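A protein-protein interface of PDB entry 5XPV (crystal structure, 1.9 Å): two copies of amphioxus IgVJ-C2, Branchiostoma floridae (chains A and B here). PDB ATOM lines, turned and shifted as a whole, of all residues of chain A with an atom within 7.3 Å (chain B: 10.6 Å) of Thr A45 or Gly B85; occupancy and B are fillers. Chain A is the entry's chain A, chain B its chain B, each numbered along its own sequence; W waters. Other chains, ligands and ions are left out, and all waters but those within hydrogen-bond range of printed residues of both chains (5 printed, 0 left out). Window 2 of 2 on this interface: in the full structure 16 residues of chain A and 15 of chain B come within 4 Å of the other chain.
The side-chain amide oxygen (OD1) of Asn A35 sits at hydrogen-bond distance from the backbone NH (N) of Gly B83 (2.9 Å).
O of Met A34 is in hydrogen-bond range of OG of Ser A32 (3.3 Å).
O of Ser A32 lies within hydrogen-bond range of OG1 of Thr A45 (2.8 Å).
O of Val A33 sits at hydrogen-bond distance from N of Thr A45 (2.8 Å).
The backbone carbonyl oxygen (O) of Asn A35 sits at hydrogen-bond distance from the backbone NH (N) of Ala A43 (2.9 Å).
The backbone carbonyl oxygen of Thr B21 is in hydrogen-bond range of the backbone NH of Ile B82.
N of Glu B81 is in hydrogen-bond range of O of Gln B87, 2.8 Å away.
Among the printed residues, pairs that only touch across the chains: Ala A43 with Gly B83 (3.4 Å), Asn A25 with Ile B80 (3.4 Å), Asn A35 with Ile B82 (3.5 Å), Asn A35 with Glu B81 (3.5 Å), Thr A45 with Gly B85 (3.7 Å), Thr A45 with Gly B86 (3.8 Å), Ser A32 with Ser B88 (3.8 Å), Ala A43 with Ala B84 (3.8 Å) and Asn A35 with Gly B86 (3.8 Å).
Of chain B, only Gly B85 (3.7 Å) and Gly B86 (3.8 Å) come within 4 Å of Thr A45.
No residue of chain B comes within 4 Å of Glu A46.
No residue of chain B comes within 4 Å of Leu A48.
No residue of chain B comes within 4 Å of Asp A49.
Printed residues of chain A within 4 Å of Ser B88: Ser A32.
Printed residues of chain A within 4 Å of Gly B86: Asn A35 and Thr A45.
Of the printed residues of chain A, Ala B84 touches Ala A43.
Of the printed residues of chain A, Ile B82 touches Asn A35 (3.5 Å).
Printed residues of chain A within 4 Å of Gly B83: Asn A35 (2.9 Å) and Ala A43 (3.4 Å).
Asp A47 touches none of the printed residues of chain B.
Tyr B15 touches none of the printed residues of chain A.
The nearest residue of chain B that does not touch Thr A45 is Gly B83 (4.6 Å).
The nearest residue of chain A that does not touch Gly B85 is Phe A44 (5.1 Å).
The nearest printed residue of chain A that does not touch Glu B81 is Asn A25 (5.2 Å).
Hydrophobic or aromatic side chains of chain A within 4 Å of the printed part of chain B: Ala A43.
Of the 17 printed residues of chain B, 8 touch a printed residue of chain A.
Hydrophobic or aromatic side chains of chain B within 4 Å of the printed part of chain A: Ile B80.
Among the printed residues, no Asp or Glu carboxylate lies within 4 Å of a Lys or Arg side-chain nitrogen of the other chain.
No position is printed for both chains.
Of the 10 pairs that touch across the chains among the printed residues, none has its exchanged pair printed and touching as well.
Water W5 lies within hydrogen-bond range of the side-chain hydroxyl of Ser A32 (2.7 Å), the side-chain hydroxyl of Thr A45 (2.7 Å), the backbone carbonyl oxygen of Gly B86 (2.9 Å) and the side-chain amide nitrogen of Asn A35 (3.0 Å).
Water W2 lies within hydrogen-bond range of the backbone carbonyl oxygen (O) of Phe A44 (2.7 Å) and the backbone NH (N) of Gly B85 (3.0 Å).
Water W1 lies within hydrogen-bond range of O of Glu B81 (2.7 Å), ND2 of Asn A25 (3.0 Å) and O of Gln B87 (3.1 Å).
Water W4 bridges OD1 of Asn A35 (2.8 Å) and N of Gly B83 (3.5 Å).
Water W3 bridges the side-chain hydroxyl of Ser B88 (2.9 Å) and the backbone NH of Ser A32 (2.9 Å).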
ATOM      1  N   ASN A  25      14.563   2.367 -11.456  1.00  0.00           N
ATOM      2  CA  ASN A  25      14.494   2.823 -10.070  1.00  0.00           C
ATOM      3  C   ASN A  25      14.053   4.276  -9.994  1.00  0.00           C
ATOM      4  O   ASN A  25      14.414   5.078 -10.854  1.00  0.00           O
ATOM      5  CB  ASN A  25      15.848   2.685  -9.365  1.00  0.00           C
ATOM      6  CG  ASN A  25      16.196   1.248  -9.036  1.00  0.00           C
ATOM      7  OD1 ASN A  25      16.393   0.431  -9.934  1.00  0.00           O
ATOM      8  ND2 ASN A  25      16.291   0.936  -7.742  1.00  0.00           N
ATOM      9  N   TRP A  26      13.291   4.608  -8.961  1.00  0.00           N
ATOM     10  CA  TRP A  26      13.021   6.004  -8.640  1.00  0.00           C
ATOM     11  C   TRP A  26      13.812   6.356  -7.389  1.00  0.00           C
ATOM     12  O   TRP A  26      13.853   5.581  -6.428  1.00  0.00           O
ATOM     13  CB  TRP A  26      11.517   6.255  -8.448  1.00  0.00           C
ATOM     14  CG  TRP A  26      10.841   6.563  -9.747  1.00  0.00           C
ATOM     15  CD1 TRP A  26      10.165   5.695 -10.548  1.00  0.00           C
ATOM     16  CD2 TRP A  26      10.824   7.828 -10.416  1.00  0.00           C
ATOM     17  NE1 TRP A  26       9.711   6.344 -11.674  1.00  0.00           N
ATOM     18  CE2 TRP A  26      10.109   7.656 -11.620  1.00  0.00           C
ATOM     19  CE3 TRP A  26      11.343   9.092 -10.115  1.00  0.00           C
ATOM     20  CZ2 TRP A  26       9.887   8.701 -12.515  1.00  0.00           C
ATOM     21  CZ3 TRP A  26      11.130  10.130 -11.010  1.00  0.00           C
ATOM     22  CH2 TRP A  26      10.408   9.925 -12.196  1.00  0.00           C
ATOM     23  N   THR A  31      18.454   8.231  -2.718  1.00  0.00           N
ATOM     24  CA  THR A  31      18.103   6.928  -2.156  1.00  0.00           C
ATOM     25  C   THR A  31      16.947   6.298  -2.927  1.00  0.00           C
ATOM     26  O   THR A  31      15.944   6.964  -3.192  1.00  0.00           O
ATOM     27  CB  THR A  31      17.709   7.038  -0.666  1.00  0.00           C
ATOM     28  OG1 THR A  31      18.815   7.556   0.084  1.00  0.00           O
ATOM     29  CG2 THR A  31      17.320   5.679  -0.112  1.00  0.00           C
ATOM     30  N   SER A  32      17.074   5.021  -3.279  1.00  0.00           N
ATOM     31  CA  SER A  32      16.031   4.360  -4.063  1.00  0.00           C
ATOM     32  C   SER A  32      14.738   4.209  -3.266  1.00  0.00           C
ATOM     33  O   SER A  32      14.735   3.615  -2.178  1.00  0.00           O
ATOM     34  CB  SER A  32      16.499   2.991  -4.543  1.00  0.00           C
ATOM     35  OG  SER A  32      15.473   2.340  -5.278  1.00  0.00           O
ATOM     36  N   VAL A  33      13.646   4.743  -3.808  1.00  0.00           N
ATOM     37  CA  VAL A  33      12.334   4.606  -3.176  1.00  0.00           C
ATOM     38  C   VAL A  33      11.438   3.658  -3.964  1.00  0.00           C
ATOM     39  O   VAL A  33      10.298   3.410  -3.583  1.00  0.00           O
ATOM     40  CB  VAL A  33      11.620   5.968  -3.025  1.00  0.00           C
ATOM     41  CG1 VAL A  33      12.306   6.807  -1.956  1.00  0.00           C
ATOM     42  CG2 VAL A  33      11.576   6.713  -4.369  1.00  0.00           C
ATOM     43  N   MET A  34      11.953   3.131  -5.068  1.00  0.00           N
ATOM     44  CA  MET A  34      11.212   2.141  -5.848  1.00  0.00           C
ATOM     45  C   MET A  34      12.125   1.433  -6.831  1.00  0.00           C
ATOM     46  O   MET A  34      12.967   2.062  -7.453  1.00  0.00           O
ATOM     47  CB  MET A  34      10.054   2.783  -6.618  1.00  0.00           C
ATOM     48  CG  MET A  34       9.074   1.766  -7.205  1.00  0.00           C
ATOM     49  SD  MET A  34       8.475   2.172  -8.867  1.00  0.00           S
ATOM     50  CE  MET A  34       9.950   1.818  -9.820  1.00  0.00           C
ATOM     51  N   ASN A  35      11.944   0.123  -6.971  1.00  0.00           N
ATOM     52  CA  ASN A  35      12.659  -0.630  -7.989  1.00  0.00           C
ATOM     53  C   ASN A  35      11.683  -1.491  -8.780  1.00  0.00           C
ATOM     54  O   ASN A  35      10.643  -1.897  -8.268  1.00  0.00           O
ATOM     55  CB  ASN A  35      13.763  -1.493  -7.363  1.00  0.00           C
ATOM     56  CG  ASN A  35      13.214  -2.567  -6.451  1.00  0.00           C
ATOM     57  OD1 ASN A  35      12.734  -3.598  -6.919  1.00  0.00           O
ATOM     58  ND2 ASN A  35      13.272  -2.331  -5.141  1.00  0.00           N
ATOM     59  N   ALA A  43       8.381  -2.348  -6.495  1.00  0.00           N
ATOM     60  CA  ALA A  43       8.560  -2.486  -5.061  1.00  0.00           C
ATOM     61  C   ALA A  43       8.941  -1.137  -4.484  1.00  0.00           C
ATOM     62  O   ALA A  43       9.997  -0.601  -4.804  1.00  0.00           O
ATOM     63  CB  ALA A  43       9.626  -3.531  -4.743  1.00  0.00           C
ATOM     64  N   PHE A  44       8.078  -0.587  -3.636  1.00  0.00           N
ATOM     65  CA  PHE A  44       8.335   0.719  -3.042  1.00  0.00           C
ATOM     66  C   PHE A  44       9.110   0.570  -1.736  1.00  0.00           C
ATOM     67  O   PHE A  44       8.832  -0.319  -0.932  1.00  0.00           O
ATOM     68  CB  PHE A  44       7.021   1.477  -2.833  1.00  0.00           C
ATOM     69  CG  PHE A  44       6.381   1.925  -4.124  1.00  0.00           C
ATOM     70  CD1 PHE A  44       5.427   1.140  -4.752  1.00  0.00           C
ATOM     71  CD2 PHE A  44       6.765   3.114  -4.725  1.00  0.00           C
ATOM     72  CE1 PHE A  44       4.848   1.544  -5.955  1.00  0.00           C
ATOM     73  CE2 PHE A  44       6.193   3.524  -5.933  1.00  0.00           C
ATOM     74  CZ  PHE A  44       5.236   2.735  -6.547  1.00  0.00           C
ATOM     75  N   THR A  45      10.098   1.440  -1.545  1.00  0.00           N
ATOM     76  CA  THR A  45      11.063   1.281  -0.467  1.00  0.00           C
ATOM     77  C   THR A  45      11.382   2.593   0.242  1.00  0.00           C
ATOM     78  O   THR A  45      11.042   3.672  -0.239  1.00  0.00           O
ATOM     79  CB  THR A  45      12.386   0.678  -0.993  1.00  0.00           C
ATOM     80  OG1 THR A  45      12.881   1.487  -2.067  1.00  0.00           O
ATOM     81  CG2 THR A  45      12.165  -0.740  -1.506  1.00  0.00           C
ATOM     82  N   GLU A  46      12.064   2.475   1.381  1.00  0.00           N
ATOM     83  CA  GLU A  46      12.485   3.612   2.205  1.00  0.00           C
ATOM     84  C   GLU A  46      11.287   4.530   2.480  1.00  0.00           C
ATOM     85  O   GLU A  46      10.275   4.067   2.984  1.00  0.00           O
ATOM     86  CB  GLU A  46      13.630   4.388   1.541  1.00  0.00           C
ATOM     87  CG  GLU A  46      14.447   5.200   2.550  1.00  0.00           C
ATOM     88  CD  GLU A  46      14.875   6.568   2.044  1.00  0.00           C
ATOM     89  OE1 GLU A  46      14.145   7.175   1.231  1.00  0.00           O
ATOM     90  OE2 GLU A  46      15.940   7.049   2.485  1.00  0.00           O
ATOM     91  N   ASP A  47      11.379   5.810   2.120  1.00  0.00           N
ATOM     92  CA  ASP A  47      10.315   6.764   2.445  1.00  0.00           C
ATOM     93  C   ASP A  47       8.967   6.452   1.797  1.00  0.00           C
ATOM     94  O   ASP A  47       7.934   6.882   2.298  1.00  0.00           O
ATOM     95  CB  ASP A  47      10.728   8.182   2.063  1.00  0.00           C
ATOM     96  CG  ASP A  47      11.739   8.772   3.022  1.00  0.00           C
ATOM     97  OD1 ASP A  47      12.092   8.101   4.017  1.00  0.00           O
ATOM     98  OD2 ASP A  47      12.162   9.921   2.788  1.00  0.00           O
ATOM     99  N   LEU A  48       8.972   5.719   0.690  1.00  0.00           N
ATOM    100  CA  LEU A  48       7.727   5.407  -0.008  1.00  0.00           C
ATOM    101  C   LEU A  48       7.199   4.032   0.375  1.00  0.00           C
ATOM    102  O   LEU A  48       6.202   3.556  -0.175  1.00  0.00           O
ATOM    103  CB  LEU A  48       7.918   5.495  -1.524  1.00  0.00           C
ATOM    104  CG  LEU A  48       8.117   6.907  -2.079  1.00  0.00           C
ATOM    105  CD1 LEU A  48       8.028   6.908  -3.597  1.00  0.00           C
ATOM    106  CD2 LEU A  48       7.126   7.903  -1.472  1.00  0.00           C
ATOM    107  N   ASP A  49       7.869   3.388   1.320  1.00  0.00           N
ATOM    108  CA  ASP A  49       7.378   2.115   1.819  1.00  0.00           C
ATOM    109  C   ASP A  49       6.155   2.390   2.688  1.00  0.00           C
ATOM    110  O   ASP A  49       6.007   3.494   3.223  1.00  0.00           O
ATOM    111  CB  ASP A  49       8.458   1.372   2.601  1.00  0.00           C
ATOM    112  CG  ASP A  49       8.174  -0.111   2.715  1.00  0.00           C
ATOM    113  OD1 ASP A  49       7.117  -0.553   2.212  1.00  0.00           O
ATOM    114  OD2 ASP A  49       9.006  -0.831   3.305  1.00  0.00           O
ATOM    115  N   ASP A  50       5.267   1.407   2.785  1.00  0.00           N
ATOM    116  CA  ASP A  50       4.051   1.510   3.600  1.00  0.00           C
ATOM    117  C   ASP A  50       3.075   2.571   3.086  1.00  0.00           C
ATOM    118  O   ASP A  50       2.016   2.783   3.677  1.00  0.00           O
ATOM    119  CB  ASP A  50       4.401   1.820   5.060  1.00  0.00           C
ATOM    120  CG  ASP A  50       5.250   0.739   5.701  1.00  0.00           C
ATOM    121  OD1 ASP A  50       5.308  -0.383   5.154  1.00  0.00           O
ATOM    122  OD2 ASP A  50       5.863   1.014   6.756  1.00  0.00           O
ATOM    123  N   TYR B  15      30.234  -4.455  -3.071  1.00  0.00           N
ATOM    124  CA  TYR B  15      28.879  -4.232  -2.584  1.00  0.00           C
ATOM    125  C   TYR B  15      28.255  -5.558  -2.141  1.00  0.00           C
ATOM    126  O   TYR B  15      28.230  -6.519  -2.907  1.00  0.00           O
ATOM    127  CB  TYR B  15      28.026  -3.568  -3.665  1.00  0.00           C
ATOM    128  CG  TYR B  15      26.673  -3.115  -3.167  1.00  0.00           C
ATOM    129  CD1 TYR B  15      26.486  -1.821  -2.694  1.00  0.00           C
ATOM    130  CD2 TYR B  15      25.588  -3.979  -3.158  1.00  0.00           C
ATOM    131  CE1 TYR B  15      25.254  -1.398  -2.232  1.00  0.00           C
ATOM    132  CE2 TYR B  15      24.348  -3.563  -2.695  1.00  0.00           C
ATOM    133  CZ  TYR B  15      24.191  -2.271  -2.234  1.00  0.00           C
ATOM    134  OH  TYR B  15      22.962  -1.850  -1.771  1.00  0.00           O
ATOM    135  N   PRO B  16      27.752  -5.619  -0.900  1.00  0.00           N
ATOM    136  CA  PRO B  16      27.163  -6.875  -0.420  1.00  0.00           C
ATOM    137  C   PRO B  16      25.845  -7.176  -1.130  1.00  0.00           C
ATOM    138  O   PRO B  16      24.980  -6.304  -1.199  1.00  0.00           O
ATOM    139  CB  PRO B  16      26.935  -6.618   1.080  1.00  0.00           C
ATOM    140  CG  PRO B  16      27.671  -5.341   1.393  1.00  0.00           C
ATOM    141  CD  PRO B  16      27.691  -4.559   0.119  1.00  0.00           C
ATOM    142  N   SER B  18      22.666  -9.592  -1.005  1.00  0.00           N
ATOM    143  CA  SER B  18      21.867 -10.584  -0.296  1.00  0.00           C
ATOM    144  C   SER B  18      20.600 -10.961  -1.075  1.00  0.00           C
ATOM    145  O   SER B  18      20.097 -12.074  -0.949  1.00  0.00           O
ATOM    146  CB  SER B  18      21.504 -10.061   1.099  1.00  0.00           C
ATOM    147  OG  SER B  18      20.843  -8.809   1.019  1.00  0.00           O
ATOM    148  N   ALA B  19      20.102 -10.036  -1.891  1.00  0.00           N
ATOM    149  CA  ALA B  19      18.899 -10.276  -2.688  1.00  0.00           C
ATOM    150  C   ALA B  19      19.070 -11.431  -3.672  1.00  0.00           C
ATOM    151  O   ALA B  19      20.175 -11.730  -4.118  1.00  0.00           O
ATOM    152  CB  ALA B  19      18.497  -9.010  -3.438  1.00  0.00           C
ATOM    153  N   ASP B  20      17.957 -12.072  -4.009  1.00  0.00           N
ATOM    154  CA  ASP B  20      17.954 -13.185  -4.947  1.00  0.00           C
ATOM    155  C   ASP B  20      17.989 -12.690  -6.388  1.00  0.00           C
ATOM    156  O   ASP B  20      18.618 -13.300  -7.257  1.00  0.00           O
ATOM    157  CB  ASP B  20      16.718 -14.060  -4.721  1.00  0.00           C
ATOM    158  CG  ASP B  20      16.530 -14.440  -3.259  1.00  0.00           C
ATOM    159  OD1 ASP B  20      17.451 -15.054  -2.677  1.00  0.00           O
ATOM    160  OD2 ASP B  20      15.458 -14.120  -2.696  1.00  0.00           O
ATOM    161  N   THR B  21      17.302 -11.580  -6.641  1.00  0.00           N
ATOM    162  CA  THR B  21      17.267 -11.000  -7.974  1.00  0.00           C
ATOM    163  C   THR B  21      17.920  -9.626  -7.953  1.00  0.00           C
ATOM    164  O   THR B  21      17.532  -8.759  -7.172  1.00  0.00           O
ATOM    165  CB  THR B  21      15.826 -10.881  -8.508  1.00  0.00           C
ATOM    166  OG1 THR B  21      15.217 -12.177  -8.531  1.00  0.00           O
ATOM    167  CG2 THR B  21      15.825 -10.300  -9.919  1.00  0.00           C
ATOM    168  N   VAL B  79      25.122  -1.895  -7.941  1.00  0.00           N
ATOM    169  CA  VAL B  79      24.216  -3.014  -7.761  1.00  0.00           C
ATOM    170  C   VAL B  79      22.807  -2.495  -7.536  1.00  0.00           C
ATOM    171  O   VAL B  79      22.604  -1.574  -6.750  1.00  0.00           O
ATOM    172  CB  VAL B  79      24.643  -3.888  -6.565  1.00  0.00           C
ATOM    173  CG1 VAL B  79      23.623  -4.983  -6.301  1.00  0.00           C
ATOM    174  CG2 VAL B  79      26.018  -4.481  -6.824  1.00  0.00           C
ATOM    175  N   ILE B  80      21.839  -3.071  -8.239  1.00  0.00           N
ATOM    176  CA  ILE B  80      20.438  -2.790  -7.951  1.00  0.00           C
ATOM    177  C   ILE B  80      19.761  -4.084  -7.525  1.00  0.00           C
ATOM    178  O   ILE B  80      19.757  -5.061  -8.271  1.00  0.00           O
ATOM    179  CB  ILE B  80      19.679  -2.184  -9.160  1.00  0.00           C
ATOM    180  CG1 ILE B  80      19.992  -0.693  -9.322  1.00  0.00           C
ATOM    181  CG2 ILE B  80      18.174  -2.316  -8.956  1.00  0.00           C
ATOM    182  CD1 ILE B  80      21.365  -0.382  -9.815  1.00  0.00           C
ATOM    183  N   GLU B  81      19.203  -4.089  -6.320  1.00  0.00           N
ATOM    184  CA  GLU B  81      18.446  -5.239  -5.833  1.00  0.00           C
ATOM    185  C   GLU B  81      16.979  -5.119  -6.218  1.00  0.00           C
ATOM    186  O   GLU B  81      16.386  -4.043  -6.116  1.00  0.00           O
ATOM    187  CB  GLU B  81      18.592  -5.376  -4.320  1.00  0.00           C
ATOM    188  CG  GLU B  81      20.027  -5.576  -3.880  1.00  0.00           C
ATOM    189  CD  GLU B  81      20.157  -5.806  -2.388  1.00  0.00           C
ATOM    190  OE1 GLU B  81      19.410  -5.164  -1.615  1.00  0.00           O
ATOM    191  OE2 GLU B  81      20.999  -6.642  -1.993  1.00  0.00           O
ATOM    192  N   ILE B  82      16.397  -6.226  -6.664  1.00  0.00           N
ATOM    193  CA  ILE B  82      15.022  -6.217  -7.144  1.00  0.00           C
ATOM    194  C   ILE B  82      14.101  -6.886  -6.135  1.00  0.00           C
ATOM    195  O   ILE B  82      14.382  -7.987  -5.657  1.00  0.00           O
ATOM    196  CB  ILE B  82      14.906  -6.918  -8.502  1.00  0.00           C
ATOM    197  CG1 ILE B  82      15.755  -6.186  -9.541  1.00  0.00           C
ATOM    198  CG2 ILE B  82      13.458  -6.958  -8.970  1.00  0.00           C
ATOM    199  CD1 ILE B  82      15.225  -4.819  -9.897  1.00  0.00           C
ATOM    200  N   GLY B  83      13.011  -6.206  -5.795  1.00  0.00           N
ATOM    201  CA  GLY B  83      12.028  -6.752  -4.879  1.00  0.00           C
ATOM    202  C   GLY B  83      11.856  -5.933  -3.618  1.00  0.00           C
ATOM    203  O   GLY B  83      12.447  -4.862  -3.470  1.00  0.00           O
ATOM    204  N   ALA B  84      11.037  -6.448  -2.705  1.00  0.00           N
ATOM    205  CA  ALA B  84      10.715  -5.752  -1.465  1.00  0.00           C
ATOM    206  C   ALA B  84      11.964  -5.433  -0.658  1.00  0.00           C
ATOM    207  O   ALA B  84      12.841  -6.281  -0.484  1.00  0.00           O
ATOM    208  CB  ALA B  84       9.743  -6.580  -0.630  1.00  0.00           C
ATOM    209  N   GLY B  85      12.042  -4.196  -0.175  1.00  0.00           N
ATOM    210  CA  GLY B  85      13.193  -3.743   0.579  1.00  0.00           C
ATOM    211  C   GLY B  85      14.474  -3.663  -0.236  1.00  0.00           C
ATOM    212  O   GLY B  85      15.546  -3.428   0.313  1.00  0.00           O
ATOM    213  N   GLY B  86      14.368  -3.851  -1.548  1.00  0.00           N
ATOM    214  CA  GLY B  86      15.536  -3.809  -2.410  1.00  0.00           C
ATOM    215  C   GLY B  86      16.320  -2.517  -2.286  1.00  0.00           C
ATOM    216  O   GLY B  86      15.756  -1.427  -2.359  1.00  0.00           O
ATOM    217  N   GLN B  87      17.624  -2.643  -2.081  1.00  0.00           N
ATOM    218  CA  GLN B  87      18.507  -1.484  -2.036  1.00  0.00           C
ATOM    219  C   GLN B  87      19.310  -1.334  -3.327  1.00  0.00           C
ATOM    220  O   GLN B  87      19.288  -2.196  -4.196  1.00  0.00           O
ATOM    221  CB  GLN B  87      19.475  -1.588  -0.856  1.00  0.00           C
ATOM    222  CG  GLN B  87      18.817  -1.666   0.510  1.00  0.00           C
ATOM    223  CD  GLN B  87      19.840  -1.833   1.616  1.00  0.00           C
ATOM    224  OE1 GLN B  87      20.397  -2.915   1.802  1.00  0.00           O
ATOM    225  NE2 GLN B  87      20.097  -0.761   2.354  1.00  0.00           N
ATOM    226  N   SER B  88      20.029  -0.229  -3.437  1.00  0.00           N
ATOM    227  CA  SER B  88      20.947  -0.039  -4.546  1.00  0.00           C
ATOM    228  C   SER B  88      22.101   0.813  -4.071  1.00  0.00           C
ATOM    229  O   SER B  88      21.948   1.616  -3.150  1.00  0.00           O
ATOM    230  CB  SER B  88      20.253   0.617  -5.739  1.00  0.00           C
ATOM    231  OG  SER B  88      20.004   1.985  -5.478  1.00  0.00           O
ATOM    232  N   GLY B  89      23.261   0.633  -4.690  1.00  0.00           N
ATOM    233  CA  GLY B  89      24.439   1.368  -4.284  1.00  0.00           C
ATOM    234  C   GLY B  89      25.636   1.067  -5.156  1.00  0.00           C
ATOM    235  O   GLY B  89      25.580   0.210  -6.041  1.00  0.00           O
HETATM  236  O   HOH W   1      16.742  -1.352  -5.782  1.00  0.00           O
HETATM  237  O   HOH W   2       9.361  -2.942  -0.365  1.00  0.00           O
HETATM  238  O   HOH W   3      19.632   3.592  -3.117  1.00  0.00           O
HETATM  239  O   HOH W   4      10.463  -5.020  -7.876  1.00  0.00           O
HETATM  240  O   HOH W   5      14.242   0.288  -4.112  1.00  0.00           O
